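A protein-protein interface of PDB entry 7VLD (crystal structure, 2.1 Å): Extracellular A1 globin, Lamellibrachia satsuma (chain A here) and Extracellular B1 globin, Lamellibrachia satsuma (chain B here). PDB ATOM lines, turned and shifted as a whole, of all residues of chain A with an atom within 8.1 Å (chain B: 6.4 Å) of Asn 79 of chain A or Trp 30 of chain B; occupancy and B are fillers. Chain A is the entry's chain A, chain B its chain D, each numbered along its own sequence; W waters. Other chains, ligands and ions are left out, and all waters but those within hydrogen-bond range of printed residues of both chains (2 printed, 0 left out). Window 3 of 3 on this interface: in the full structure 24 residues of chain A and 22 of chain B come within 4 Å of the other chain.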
ATOM      1  N   ARG A   7     -16.050  -6.463  27.129  1.00  0.00           N
ATOM      2  CA  ARG A   7     -17.003  -6.342  26.028  1.00  0.00           C
ATOM      3  C   ARG A   7     -17.874  -5.102  26.187  1.00  0.00           C
ATOM      4  O   ARG A   7     -18.132  -4.388  25.211  1.00  0.00           O
ATOM      5  CB  ARG A   7     -17.869  -7.600  25.939  1.00  0.00           C
ATOM      6  CG  ARG A   7     -17.124  -8.818  25.423  1.00  0.00           C
ATOM      7  CD  ARG A   7     -17.919 -10.108  25.570  1.00  0.00           C
ATOM      8  NE  ARG A   7     -17.095 -11.281  25.283  1.00  0.00           N
ATOM      9  CZ  ARG A   7     -17.282 -12.104  24.255  1.00  0.00           C
ATOM     10  NH1 ARG A   7     -18.282 -11.901  23.407  1.00  0.00           N
ATOM     11  NH2 ARG A   7     -16.473 -13.141  24.081  1.00  0.00           N
ATOM     12  N   LYS A  11     -17.768  -1.760  23.915  1.00  0.00           N
ATOM     13  CA  LYS A  11     -19.033  -1.296  23.353  1.00  0.00           C
ATOM     14  C   LYS A  11     -19.227   0.200  23.578  1.00  0.00           C
ATOM     15  O   LYS A  11     -19.710   0.913  22.690  1.00  0.00           O
ATOM     16  CB  LYS A  11     -20.181  -2.092  23.970  1.00  0.00           C
ATOM     17  CG  LYS A  11     -21.404  -2.247  23.091  1.00  0.00           C
ATOM     18  CD  LYS A  11     -22.053  -3.597  23.352  1.00  0.00           C
ATOM     19  CE  LYS A  11     -23.528  -3.583  23.011  1.00  0.00           C
ATOM     20  NZ  LYS A  11     -24.243  -4.788  23.507  1.00  0.00           N
ATOM     21  N   VAL A  73     -21.388  -6.413  14.911  1.00  0.00           N
ATOM     22  CA  VAL A  73     -20.681  -7.456  15.646  1.00  0.00           C
ATOM     23  C   VAL A  73     -20.398  -7.003  17.074  1.00  0.00           C
ATOM     24  O   VAL A  73     -20.608  -7.752  18.035  1.00  0.00           O
ATOM     25  CB  VAL A  73     -19.383  -7.843  14.911  1.00  0.00           C
ATOM     26  CG1 VAL A  73     -18.472  -8.646  15.825  1.00  0.00           C
ATOM     27  CG2 VAL A  73     -19.700  -8.630  13.645  1.00  0.00           C
ATOM     28  N   ILE A  74     -19.916  -5.768  17.229  1.00  0.00           N
ATOM     29  CA  ILE A  74     -19.678  -5.221  18.562  1.00  0.00           C
ATOM     30  C   ILE A  74     -20.980  -5.160  19.352  1.00  0.00           C
ATOM     31  O   ILE A  74     -21.008  -5.445  20.556  1.00  0.00           O
ATOM     32  CB  ILE A  74     -19.005  -3.838  18.457  1.00  0.00           C
ATOM     33  CG1 ILE A  74     -17.574  -3.983  17.928  1.00  0.00           C
ATOM     34  CG2 ILE A  74     -19.018  -3.121  19.802  1.00  0.00           C
ATOM     35  CD1 ILE A  74     -16.858  -2.667  17.711  1.00  0.00           C
ATOM     36  N   SER A  75     -22.083  -4.811  18.684  1.00  0.00           N
ATOM     37  CA  SER A  75     -23.365  -4.716  19.376  1.00  0.00           C
ATOM     38  C   SER A  75     -23.824  -6.070  19.901  1.00  0.00           C
ATOM     39  O   SER A  75     -24.523  -6.136  20.919  1.00  0.00           O
ATOM     40  CB  SER A  75     -24.427  -4.122  18.449  1.00  0.00           C
ATOM     41  OG  SER A  75     -24.954  -5.106  17.575  1.00  0.00           O
ATOM     42  N   MET A  76     -23.444  -7.155  19.228  1.00  0.00           N
ATOM     43  CA  MET A  76     -23.805  -8.503  19.645  1.00  0.00           C
ATOM     44  C   MET A  76     -22.772  -9.133  20.575  1.00  0.00           C
ATOM     45  O   MET A  76     -22.811 -10.350  20.787  1.00  0.00           O
ATOM     46  CB  MET A  76     -24.012  -9.398  18.419  1.00  0.00           C
ATOM     47  CG  MET A  76     -25.269  -9.081  17.621  1.00  0.00           C
ATOM     48  SD  MET A  76     -25.471 -10.131  16.167  1.00  0.00           S
ATOM     49  CE  MET A  76     -24.159  -9.511  15.117  1.00  0.00           C
ATOM     50  N   PHE A  77     -21.857  -8.334  21.134  1.00  0.00           N
ATOM     51  CA  PHE A  77     -20.833  -8.877  22.023  1.00  0.00           C
ATOM     52  C   PHE A  77     -21.443  -9.579  23.231  1.00  0.00           C
ATOM     53  O   PHE A  77     -20.835 -10.506  23.778  1.00  0.00           O
ATOM     54  CB  PHE A  77     -19.891  -7.763  22.488  1.00  0.00           C
ATOM     55  CG  PHE A  77     -18.593  -7.697  21.726  1.00  0.00           C
ATOM     56  CD1 PHE A  77     -18.172  -8.761  20.946  1.00  0.00           C
ATOM     57  CD2 PHE A  77     -17.789  -6.571  21.802  1.00  0.00           C
ATOM     58  CE1 PHE A  77     -16.976  -8.699  20.250  1.00  0.00           C
ATOM     59  CE2 PHE A  77     -16.594  -6.504  21.110  1.00  0.00           C
ATOM     60  CZ  PHE A  77     -16.186  -7.569  20.333  1.00  0.00           C
ATOM     61  N   ASP A  78     -22.634  -9.164  23.655  1.00  0.00           N
ATOM     62  CA  ASP A  78     -23.262  -9.708  24.852  1.00  0.00           C
ATOM     63  C   ASP A  78     -24.120 -10.940  24.582  1.00  0.00           C
ATOM     64  O   ASP A  78     -24.638 -11.531  25.534  1.00  0.00           O
ATOM     65  CB  ASP A  78     -24.106  -8.629  25.541  1.00  0.00           C
ATOM     66  CG  ASP A  78     -25.060  -7.927  24.590  1.00  0.00           C
ATOM     67  OD1 ASP A  78     -25.236  -8.402  23.448  1.00  0.00           O
ATOM     68  OD2 ASP A  78     -25.632  -6.889  24.986  1.00  0.00           O
ATOM     69  N   ASN A  79     -24.282 -11.347  23.323  1.00  0.00           N
ATOM     70  CA  ASN A  79     -25.063 -12.534  22.976  1.00  0.00           C
ATOM     71  C   ASN A  79     -24.188 -13.454  22.129  1.00  0.00           C
ATOM     72  O   ASN A  79     -23.987 -13.203  20.937  1.00  0.00           O
ATOM     73  CB  ASN A  79     -26.347 -12.163  22.243  1.00  0.00           C
ATOM     74  CG  ASN A  79     -27.318 -13.325  22.150  1.00  0.00           C
ATOM     75  OD1 ASN A  79     -27.284 -14.105  21.199  1.00  0.00           O
ATOM     76  ND2 ASN A  79     -28.186 -13.449  23.148  1.00  0.00           N
ATOM     77  N   GLU A  80     -23.688 -14.526  22.750  1.00  0.00           N
ATOM     78  CA  GLU A  80     -22.773 -15.437  22.065  1.00  0.00           C
ATOM     79  C   GLU A  80     -23.432 -16.101  20.862  1.00  0.00           C
ATOM     80  O   GLU A  80     -22.811 -16.230  19.800  1.00  0.00           O
ATOM     81  CB  GLU A  80     -22.267 -16.497  23.044  1.00  0.00           C
ATOM     82  CG  GLU A  80     -21.194 -16.007  23.996  1.00  0.00           C
ATOM     83  CD  GLU A  80     -19.807 -16.083  23.392  1.00  0.00           C
ATOM     84  OE1 GLU A  80     -19.484 -17.118  22.774  1.00  0.00           O
ATOM     85  OE2 GLU A  80     -19.042 -15.106  23.532  1.00  0.00           O
ATOM     86  N   ASP A  81     -24.685 -16.538  21.012  1.00  0.00           N
ATOM     87  CA  ASP A  81     -25.360 -17.261  19.936  1.00  0.00           C
ATOM     88  C   ASP A  81     -25.467 -16.406  18.679  1.00  0.00           C
ATOM     89  O   ASP A  81     -25.135 -16.859  17.577  1.00  0.00           O
ATOM     90  CB  ASP A  81     -26.744 -17.717  20.398  1.00  0.00           C
ATOM     91  CG  ASP A  81     -26.680 -18.747  21.510  1.00  0.00           C
ATOM     92  OD1 ASP A  81     -25.735 -19.563  21.514  1.00  0.00           O
ATOM     93  OD2 ASP A  81     -27.578 -18.741  22.378  1.00  0.00           O
ATOM     94  N   ALA A  82     -25.930 -15.163  18.825  1.00  0.00           N
ATOM     95  CA  ALA A  82     -26.039 -14.282  17.668  1.00  0.00           C
ATOM     96  C   ALA A  82     -24.664 -13.859  17.162  1.00  0.00           C
ATOM     97  O   ALA A  82     -24.442 -13.780  15.949  1.00  0.00           O
ATOM     98  CB  ALA A  82     -26.885 -13.058  18.017  1.00  0.00           C
ATOM     99  N   LEU A  83     -23.732 -13.589  18.080  1.00  0.00           N
ATOM    100  CA  LEU A  83     -22.390 -13.168  17.682  1.00  0.00           C
ATOM    101  C   LEU A  83     -21.703 -14.234  16.838  1.00  0.00           C
ATOM    102  O   LEU A  83     -21.182 -13.944  15.756  1.00  0.00           O
ATOM    103  CB  LEU A  83     -21.555 -12.847  18.923  1.00  0.00           C
ATOM    104  CG  LEU A  83     -20.056 -12.616  18.708  1.00  0.00           C
ATOM    105  CD1 LEU A  83     -19.817 -11.381  17.856  1.00  0.00           C
ATOM    106  CD2 LEU A  83     -19.329 -12.506  20.040  1.00  0.00           C
ATOM    107  N   ASN A  84     -21.696 -15.479  17.316  1.00  0.00           N
ATOM    108  CA  ASN A  84     -21.000 -16.540  16.595  1.00  0.00           C
ATOM    109  C   ASN A  84     -21.679 -16.845  15.267  1.00  0.00           C
ATOM    110  O   ASN A  84     -21.004 -17.159  14.280  1.00  0.00           O
ATOM    111  CB  ASN A  84     -20.912 -17.793  17.462  1.00  0.00           C
ATOM    112  CG  ASN A  84     -19.941 -17.632  18.613  1.00  0.00           C
ATOM    113  OD1 ASN A  84     -18.876 -17.033  18.459  1.00  0.00           O
ATOM    114  ND2 ASN A  84     -20.307 -18.157  19.776  1.00  0.00           N
ATOM    115  N   ALA A  85     -23.009 -16.753  15.218  1.00  0.00           N
ATOM    116  CA  ALA A  85     -23.712 -16.965  13.958  1.00  0.00           C
ATOM    117  C   ALA A  85     -23.300 -15.928  12.919  1.00  0.00           C
ATOM    118  O   ALA A  85     -23.053 -16.266  11.756  1.00  0.00           O
ATOM    119  CB  ALA A  85     -25.223 -16.933  14.185  1.00  0.00           C
ATOM    120  N   ASP A  86     -23.201 -14.659  13.325  1.00  0.00           N
ATOM    121  CA  ASP A  86     -22.812 -13.619  12.378  1.00  0.00           C
ATOM    122  C   ASP A  86     -21.335 -13.725  12.017  1.00  0.00           C
ATOM    123  O   ASP A  86     -20.953 -13.468  10.870  1.00  0.00           O
ATOM    124  CB  ASP A  86     -23.138 -12.239  12.950  1.00  0.00           C
ATOM    125  CG  ASP A  86     -23.113 -11.150  11.896  1.00  0.00           C
ATOM    126  OD1 ASP A  86     -23.618 -11.391  10.778  1.00  0.00           O
ATOM    127  OD2 ASP A  86     -22.605 -10.047  12.187  1.00  0.00           O
ATOM    128  N   GLY B  25     -28.382  -1.850  22.729  1.00  0.00           N
ATOM    129  CA  GLY B  25     -28.071  -3.257  22.896  1.00  0.00           C
ATOM    130  C   GLY B  25     -28.661  -4.100  21.782  1.00  0.00           C
ATOM    131  O   GLY B  25     -29.673  -3.749  21.170  1.00  0.00           O
ATOM    132  N   ALA B  26     -28.010  -5.236  21.516  1.00  0.00           N
ATOM    133  CA  ALA B  26     -28.454  -6.105  20.431  1.00  0.00           C
ATOM    134  C   ALA B  26     -29.829  -6.700  20.704  1.00  0.00           C
ATOM    135  O   ALA B  26     -30.568  -6.996  19.758  1.00  0.00           O
ATOM    136  CB  ALA B  26     -27.434  -7.218  20.194  1.00  0.00           C
ATOM    137  N   LYS B  27     -30.187  -6.887  21.978  1.00  0.00           N
ATOM    138  CA  LYS B  27     -31.510  -7.416  22.299  1.00  0.00           C
ATOM    139  C   LYS B  27     -32.609  -6.495  21.786  1.00  0.00           C
ATOM    140  O   LYS B  27     -33.605  -6.959  21.219  1.00  0.00           O
ATOM    141  CB  LYS B  27     -31.653  -7.621  23.806  1.00  0.00           C
ATOM    142  CG  LYS B  27     -33.050  -8.068  24.216  1.00  0.00           C
ATOM    143  CD  LYS B  27     -33.287  -7.933  25.711  1.00  0.00           C
ATOM    144  CE  LYS B  27     -32.561  -9.007  26.498  1.00  0.00           C
ATOM    145  NZ  LYS B  27     -32.924  -8.953  27.942  1.00  0.00           N
ATOM    146  N   SER B  28     -32.448  -5.184  21.980  1.00  0.00           N
ATOM    147  CA  SER B  28     -33.404  -4.235  21.425  1.00  0.00           C
ATOM    148  C   SER B  28     -33.411  -4.281  19.905  1.00  0.00           C
ATOM    149  O   SER B  28     -34.463  -4.093  19.283  1.00  0.00           O
ATOM    150  CB  SER B  28     -33.082  -2.822  21.905  1.00  0.00           C
ATOM    151  OG  SER B  28     -32.836  -2.812  23.297  1.00  0.00           O
ATOM    152  N   ARG B  29     -32.249  -4.528  19.295  1.00  0.00           N
ATOM    153  CA  ARG B  29     -32.172  -4.611  17.842  1.00  0.00           C
ATOM    154  C   ARG B  29     -33.045  -5.741  17.309  1.00  0.00           C
ATOM    155  O   ARG B  29     -33.893  -5.524  16.435  1.00  0.00           O
ATOM    156  CB  ARG B  29     -30.719  -4.801  17.403  1.00  0.00           C
ATOM    157  CG  ARG B  29     -29.864  -3.542  17.454  1.00  0.00           C
ATOM    158  CD  ARG B  29     -28.387  -3.905  17.377  1.00  0.00           C
ATOM    159  NE  ARG B  29     -27.594  -2.914  16.654  1.00  0.00           N
ATOM    160  CZ  ARG B  29     -26.970  -1.889  17.225  1.00  0.00           C
ATOM    161  NH1 ARG B  29     -27.048  -1.708  18.536  1.00  0.00           N
ATOM    162  NH2 ARG B  29     -26.268  -1.043  16.484  1.00  0.00           N
ATOM    163  N   TRP B  30     -32.861  -6.957  17.827  1.00  0.00           N
ATOM    164  CA  TRP B  30     -33.618  -8.083  17.294  1.00  0.00           C
ATOM    165  C   TRP B  30     -35.054  -8.119  17.800  1.00  0.00           C
ATOM    166  O   TRP B  30     -35.900  -8.761  17.166  1.00  0.00           O
ATOM    167  CB  TRP B  30     -32.905  -9.412  17.585  1.00  0.00           C
ATOM    168  CG  TRP B  30     -32.840  -9.864  19.020  1.00  0.00           C
ATOM    169  CD1 TRP B  30     -33.887 -10.060  19.876  1.00  0.00           C
ATOM    170  CD2 TRP B  30     -31.661 -10.245  19.741  1.00  0.00           C
ATOM    171  NE1 TRP B  30     -33.429 -10.504  21.092  1.00  0.00           N
ATOM    172  CE2 TRP B  30     -32.067 -10.630  21.035  1.00  0.00           C
ATOM    173  CE3 TRP B  30     -30.300 -10.283  19.422  1.00  0.00           C
ATOM    174  CZ2 TRP B  30     -31.162 -11.045  22.008  1.00  0.00           C
ATOM    175  CZ3 TRP B  30     -29.403 -10.696  20.390  1.00  0.00           C
ATOM    176  CH2 TRP B  30     -29.838 -11.071  21.667  1.00  0.00           C
ATOM    177  N   THR B  31     -35.352  -7.457  18.922  1.00  0.00           N
ATOM    178  CA  THR B  31     -36.746  -7.266  19.307  1.00  0.00           C
ATOM    179  C   THR B  31     -37.485  -6.469  18.240  1.00  0.00           C
ATOM    180  O   THR B  31     -38.576  -6.852  17.803  1.00  0.00           O
ATOM    181  CB  THR B  31     -36.835  -6.560  20.661  1.00  0.00           C
ATOM    182  OG1 THR B  31     -36.123  -7.317  21.648  1.00  0.00           O
ATOM    183  CG2 THR B  31     -38.289  -6.418  21.092  1.00  0.00           C
ATOM    184  N   MET B  32     -36.893  -5.356  17.802  1.00  0.00           N
ATOM    185  CA  MET B  32     -37.430  -4.632  16.656  1.00  0.00           C
ATOM    186  C   MET B  32     -37.393  -5.495  15.403  1.00  0.00           C
ATOM    187  O   MET B  32     -38.356  -5.517  14.626  1.00  0.00           O
ATOM    188  CB  MET B  32     -36.644  -3.338  16.438  1.00  0.00           C
ATOM    189  CG  MET B  32     -36.756  -2.335  17.576  1.00  0.00           C
ATOM    190  SD  MET B  32     -35.691  -0.899  17.333  1.00  0.00           S
ATOM    191  CE  MET B  32     -36.037  -0.511  15.619  1.00  0.00           C
ATOM    192  N   GLY B  33     -36.292  -6.222  15.195  1.00  0.00           N
ATOM    193  CA  GLY B  33     -36.198  -7.089  14.033  1.00  0.00           C
ATOM    194  C   GLY B  33     -37.265  -8.167  14.014  1.00  0.00           C
ATOM    195  O   GLY B  33     -37.845  -8.459  12.965  1.00  0.00           O
ATOM    196  N   ASN B  34     -37.546  -8.766  15.173  1.00  0.00           N
ATOM    197  CA  ASN B  34     -38.569  -9.805  15.227  1.00  0.00           C
ATOM    198  C   ASN B  34     -39.964  -9.226  15.018  1.00  0.00           C
ATOM    199  O   ASN B  34     -40.807  -9.852  14.364  1.00  0.00           O
ATOM    200  CB  ASN B  34     -38.489 -10.562  16.553  1.00  0.00           C
ATOM    201  CG  ASN B  34     -37.419 -11.641  16.546  1.00  0.00           C
ATOM    202  OD1 ASN B  34     -36.996 -12.105  15.487  1.00  0.00           O
ATOM    203  ND2 ASN B  34     -36.984 -12.054  17.731  1.00  0.00           N
ATOM    204  N   GLU B  35     -40.227  -8.033  15.561  1.00  0.00           N
ATOM    205  CA  GLU B  35     -41.516  -7.387  15.325  1.00  0.00           C
ATOM    206  C   GLU B  35     -41.708  -7.066  13.849  1.00  0.00           C
ATOM    207  O   GLU B  35     -42.812  -7.214  13.310  1.00  0.00           O
ATOM    208  CB  GLU B  35     -41.631  -6.111  16.162  1.00  0.00           C
ATOM    209  CG  GLU B  35     -41.840  -6.348  17.645  1.00  0.00           C
ATOM    210  CD  GLU B  35     -43.198  -6.947  17.954  1.00  0.00           C
ATOM    211  OE1 GLU B  35     -44.159  -6.671  17.204  1.00  0.00           O
ATOM    212  OE2 GLU B  35     -43.304  -7.698  18.947  1.00  0.00           O
ATOM    213  N   MET B  59     -37.372 -17.913  15.502  1.00  0.00           N
ATOM    214  CA  MET B  59     -36.953 -16.516  15.496  1.00  0.00           C
ATOM    215  C   MET B  59     -36.254 -16.097  16.785  1.00  0.00           C
ATOM    216  O   MET B  59     -35.893 -14.922  16.916  1.00  0.00           O
ATOM    217  CB  MET B  59     -38.163 -15.618  15.230  1.00  0.00           C
ATOM    218  CG  MET B  59     -38.897 -15.962  13.939  1.00  0.00           C
ATOM    219  SD  MET B  59     -40.411 -15.017  13.685  1.00  0.00           S
ATOM    220  CE  MET B  59     -39.757 -13.358  13.526  1.00  0.00           C
ATOM    221  N   GLY B  62     -29.913 -17.869  17.505  1.00  0.00           N
ATOM    222  CA  GLY B  62     -28.827 -16.962  17.182  1.00  0.00           C
ATOM    223  C   GLY B  62     -28.716 -16.686  15.696  1.00  0.00           C
ATOM    224  O   GLY B  62     -28.355 -15.577  15.292  1.00  0.00           O
ATOM    225  N   PHE B  64     -31.174 -16.538  13.331  1.00  0.00           N
ATOM    226  CA  PHE B  64     -32.152 -15.560  12.866  1.00  0.00           C
ATOM    227  C   PHE B  64     -31.968 -14.214  13.554  1.00  0.00           C
ATOM    228  O   PHE B  64     -32.194 -13.170  12.931  1.00  0.00           O
ATOM    229  CB  PHE B  64     -33.574 -16.078  13.080  1.00  0.00           C
ATOM    230  CG  PHE B  64     -34.624 -15.236  12.411  1.00  0.00           C
ATOM    231  CD1 PHE B  64     -34.840 -15.333  11.046  1.00  0.00           C
ATOM    232  CD2 PHE B  64     -35.386 -14.342  13.144  1.00  0.00           C
ATOM    233  CE1 PHE B  64     -35.802 -14.557  10.425  1.00  0.00           C
ATOM    234  CE2 PHE B  64     -36.348 -13.565  12.529  1.00  0.00           C
ATOM    235  CZ  PHE B  64     -36.556 -13.672  11.168  1.00  0.00           C
ATOM    236  N   HIS B  65     -31.571 -14.214  14.831  1.00  0.00           N
ATOM    237  CA  HIS B  65     -31.233 -12.961  15.501  1.00  0.00           C
ATOM    238  C   HIS B  65     -30.155 -12.208  14.731  1.00  0.00           C
ATOM    239  O   HIS B  65     -30.269 -11.000  14.498  1.00  0.00           O
ATOM    240  CB  HIS B  65     -30.775 -13.233  16.935  1.00  0.00           C
ATOM    241  CG  HIS B  65     -31.897 -13.358  17.919  1.00  0.00           C
ATOM    242  ND1 HIS B  65     -31.710 -13.817  19.205  1.00  0.00           N
ATOM    243  CD2 HIS B  65     -33.216 -13.074  17.809  1.00  0.00           C
ATOM    244  CE1 HIS B  65     -32.866 -13.816  19.843  1.00  0.00           C
ATOM    245  NE2 HIS B  65     -33.797 -13.369  19.019  1.00  0.00           N
ATOM    246  N   ALA B  66     -29.102 -12.918  14.314  1.00  0.00           N
ATOM    247  CA  ALA B  66     -28.043 -12.284  13.538  1.00  0.00           C
ATOM    248  C   ALA B  66     -28.546 -11.805  12.185  1.00  0.00           C
ATOM    249  O   ALA B  66     -28.019 -10.828  11.640  1.00  0.00           O
ATOM    250  CB  ALA B  66     -26.873 -13.252  13.357  1.00  0.00           C
ATOM    251  N   THR B  68     -31.651 -10.506  11.478  1.00  0.00           N
ATOM    252  CA  THR B  68     -32.340  -9.231  11.649  1.00  0.00           C
ATOM    253  C   THR B  68     -31.362  -8.125  12.024  1.00  0.00           C
ATOM    254  O   THR B  68     -31.528  -6.975  11.603  1.00  0.00           O
ATOM    255  CB  THR B  68     -33.443  -9.357  12.701  1.00  0.00           C
ATOM    256  OG1 THR B  68     -32.861  -9.579  13.991  1.00  0.00           O
ATOM    257  CG2 THR B  68     -34.373 -10.513  12.358  1.00  0.00           C
ATOM    258  N   VAL B  69     -30.337  -8.456  12.811  1.00  0.00           N
ATOM    259  CA  VAL B  69     -29.274  -7.494  13.092  1.00  0.00           C
ATOM    260  C   VAL B  69     -28.582  -7.080  11.799  1.00  0.00           C
ATOM    261  O   VAL B  69     -28.265  -5.900  11.597  1.00  0.00           O
ATOM    262  CB  VAL B  69     -28.280  -8.080  14.111  1.00  0.00           C
ATOM    263  CG1 VAL B  69     -27.030  -7.218  14.200  1.00  0.00           C
ATOM    264  CG2 VAL B  69     -28.936  -8.206  15.477  1.00  0.00           C
ATOM    265  N   LEU B  72     -31.222  -4.769   9.840  1.00  0.00           N
ATOM    266  CA  LEU B  72     -31.360  -3.428  10.399  1.00  0.00           C
ATOM    267  C   LEU B  72     -30.070  -2.627  10.271  1.00  0.00           C
ATOM    268  O   LEU B  72     -30.118  -1.396  10.158  1.00  0.00           O
ATOM    269  CB  LEU B  72     -31.804  -3.516  11.859  1.00  0.00           C
ATOM    270  CG  LEU B  72     -33.184  -4.142  12.075  1.00  0.00           C
ATOM    271  CD1 LEU B  72     -33.494  -4.262  13.554  1.00  0.00           C
ATOM    272  CD2 LEU B  72     -34.268  -3.344  11.361  1.00  0.00           C
HETATM  273  O   HOH W   1     -28.438  -7.025  23.897  1.00  0.00           O
HETATM  274  O   HOH W   2     -29.489 -15.213  20.182  1.00  0.00           O
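O of Ser 75 of chain A is in hydrogen-bond range of NZ of Lys 11 of chain A (2.9 Å). N of Ala 82 of chain A lies within hydrogen-bond range of OD1 of Asn 79 of chain A (2.9 Å).
Among the printed residues, merely in contact across the chains: Ser 75 of chain A with Ala 26 of chain B, Ser 75 of chain A with Arg 29 of chain B, Met 76 of chain A with Ala 26 of chain B, Met 76 of chain A with Val 69 of chain B, Asn 79 of chain A with Trp 30 of chain B, Asp 81 of chain A with Gly 62 of chain B, Ala 82 of chain A with Gly 62 of chain B, Ala 82 of chain A with Ala 66 of chain B, Ala 85 of chain A with Gly 62 of chain B and Asp 86 of chain A with Ala 66 of chain B.
Asn 79 of chain A touches one residue of chain B. Of the printed residues of chain A, Trp 30 of chain B touches Asn 79 (3.3 Å). Printed residues of chain B within 4 Å of Ser 75 of chain A: Ala 26 (3.2 Å) and Arg 29 (3.6 Å). Printed residues of chain B within 4 Å of Ala 82 of chain A: Gly 62 (3.6 Å) and Ala 66 (3.6 Å). Printed residues of chain B within 4 Å of Asp 86 of chain A: Ala 66 (3.9 Å). Of the printed residues of chain A, Ala 66 of chain B touches Ala 82 and Asp 86. Asp 78 of chain A touches none of the printed residues of chain B. The nearest residue of chain B that does not touch Asn 79 of chain A is His 65 of chain B (4.9 Å).
Water W1 lies within hydrogen-bond range of N of Lys 27 of chain B (2.6 Å), N of Ala 26 of chain B (3.0 Å) and OD2 of Asp 78 of chain A (3.0 Å). Water W2 bridges the side-chain amide oxygen of Asn 79 of chain A (2.7 Å) and a ring nitrogen (ND1) of His 65 of chain B (2.8 Å).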
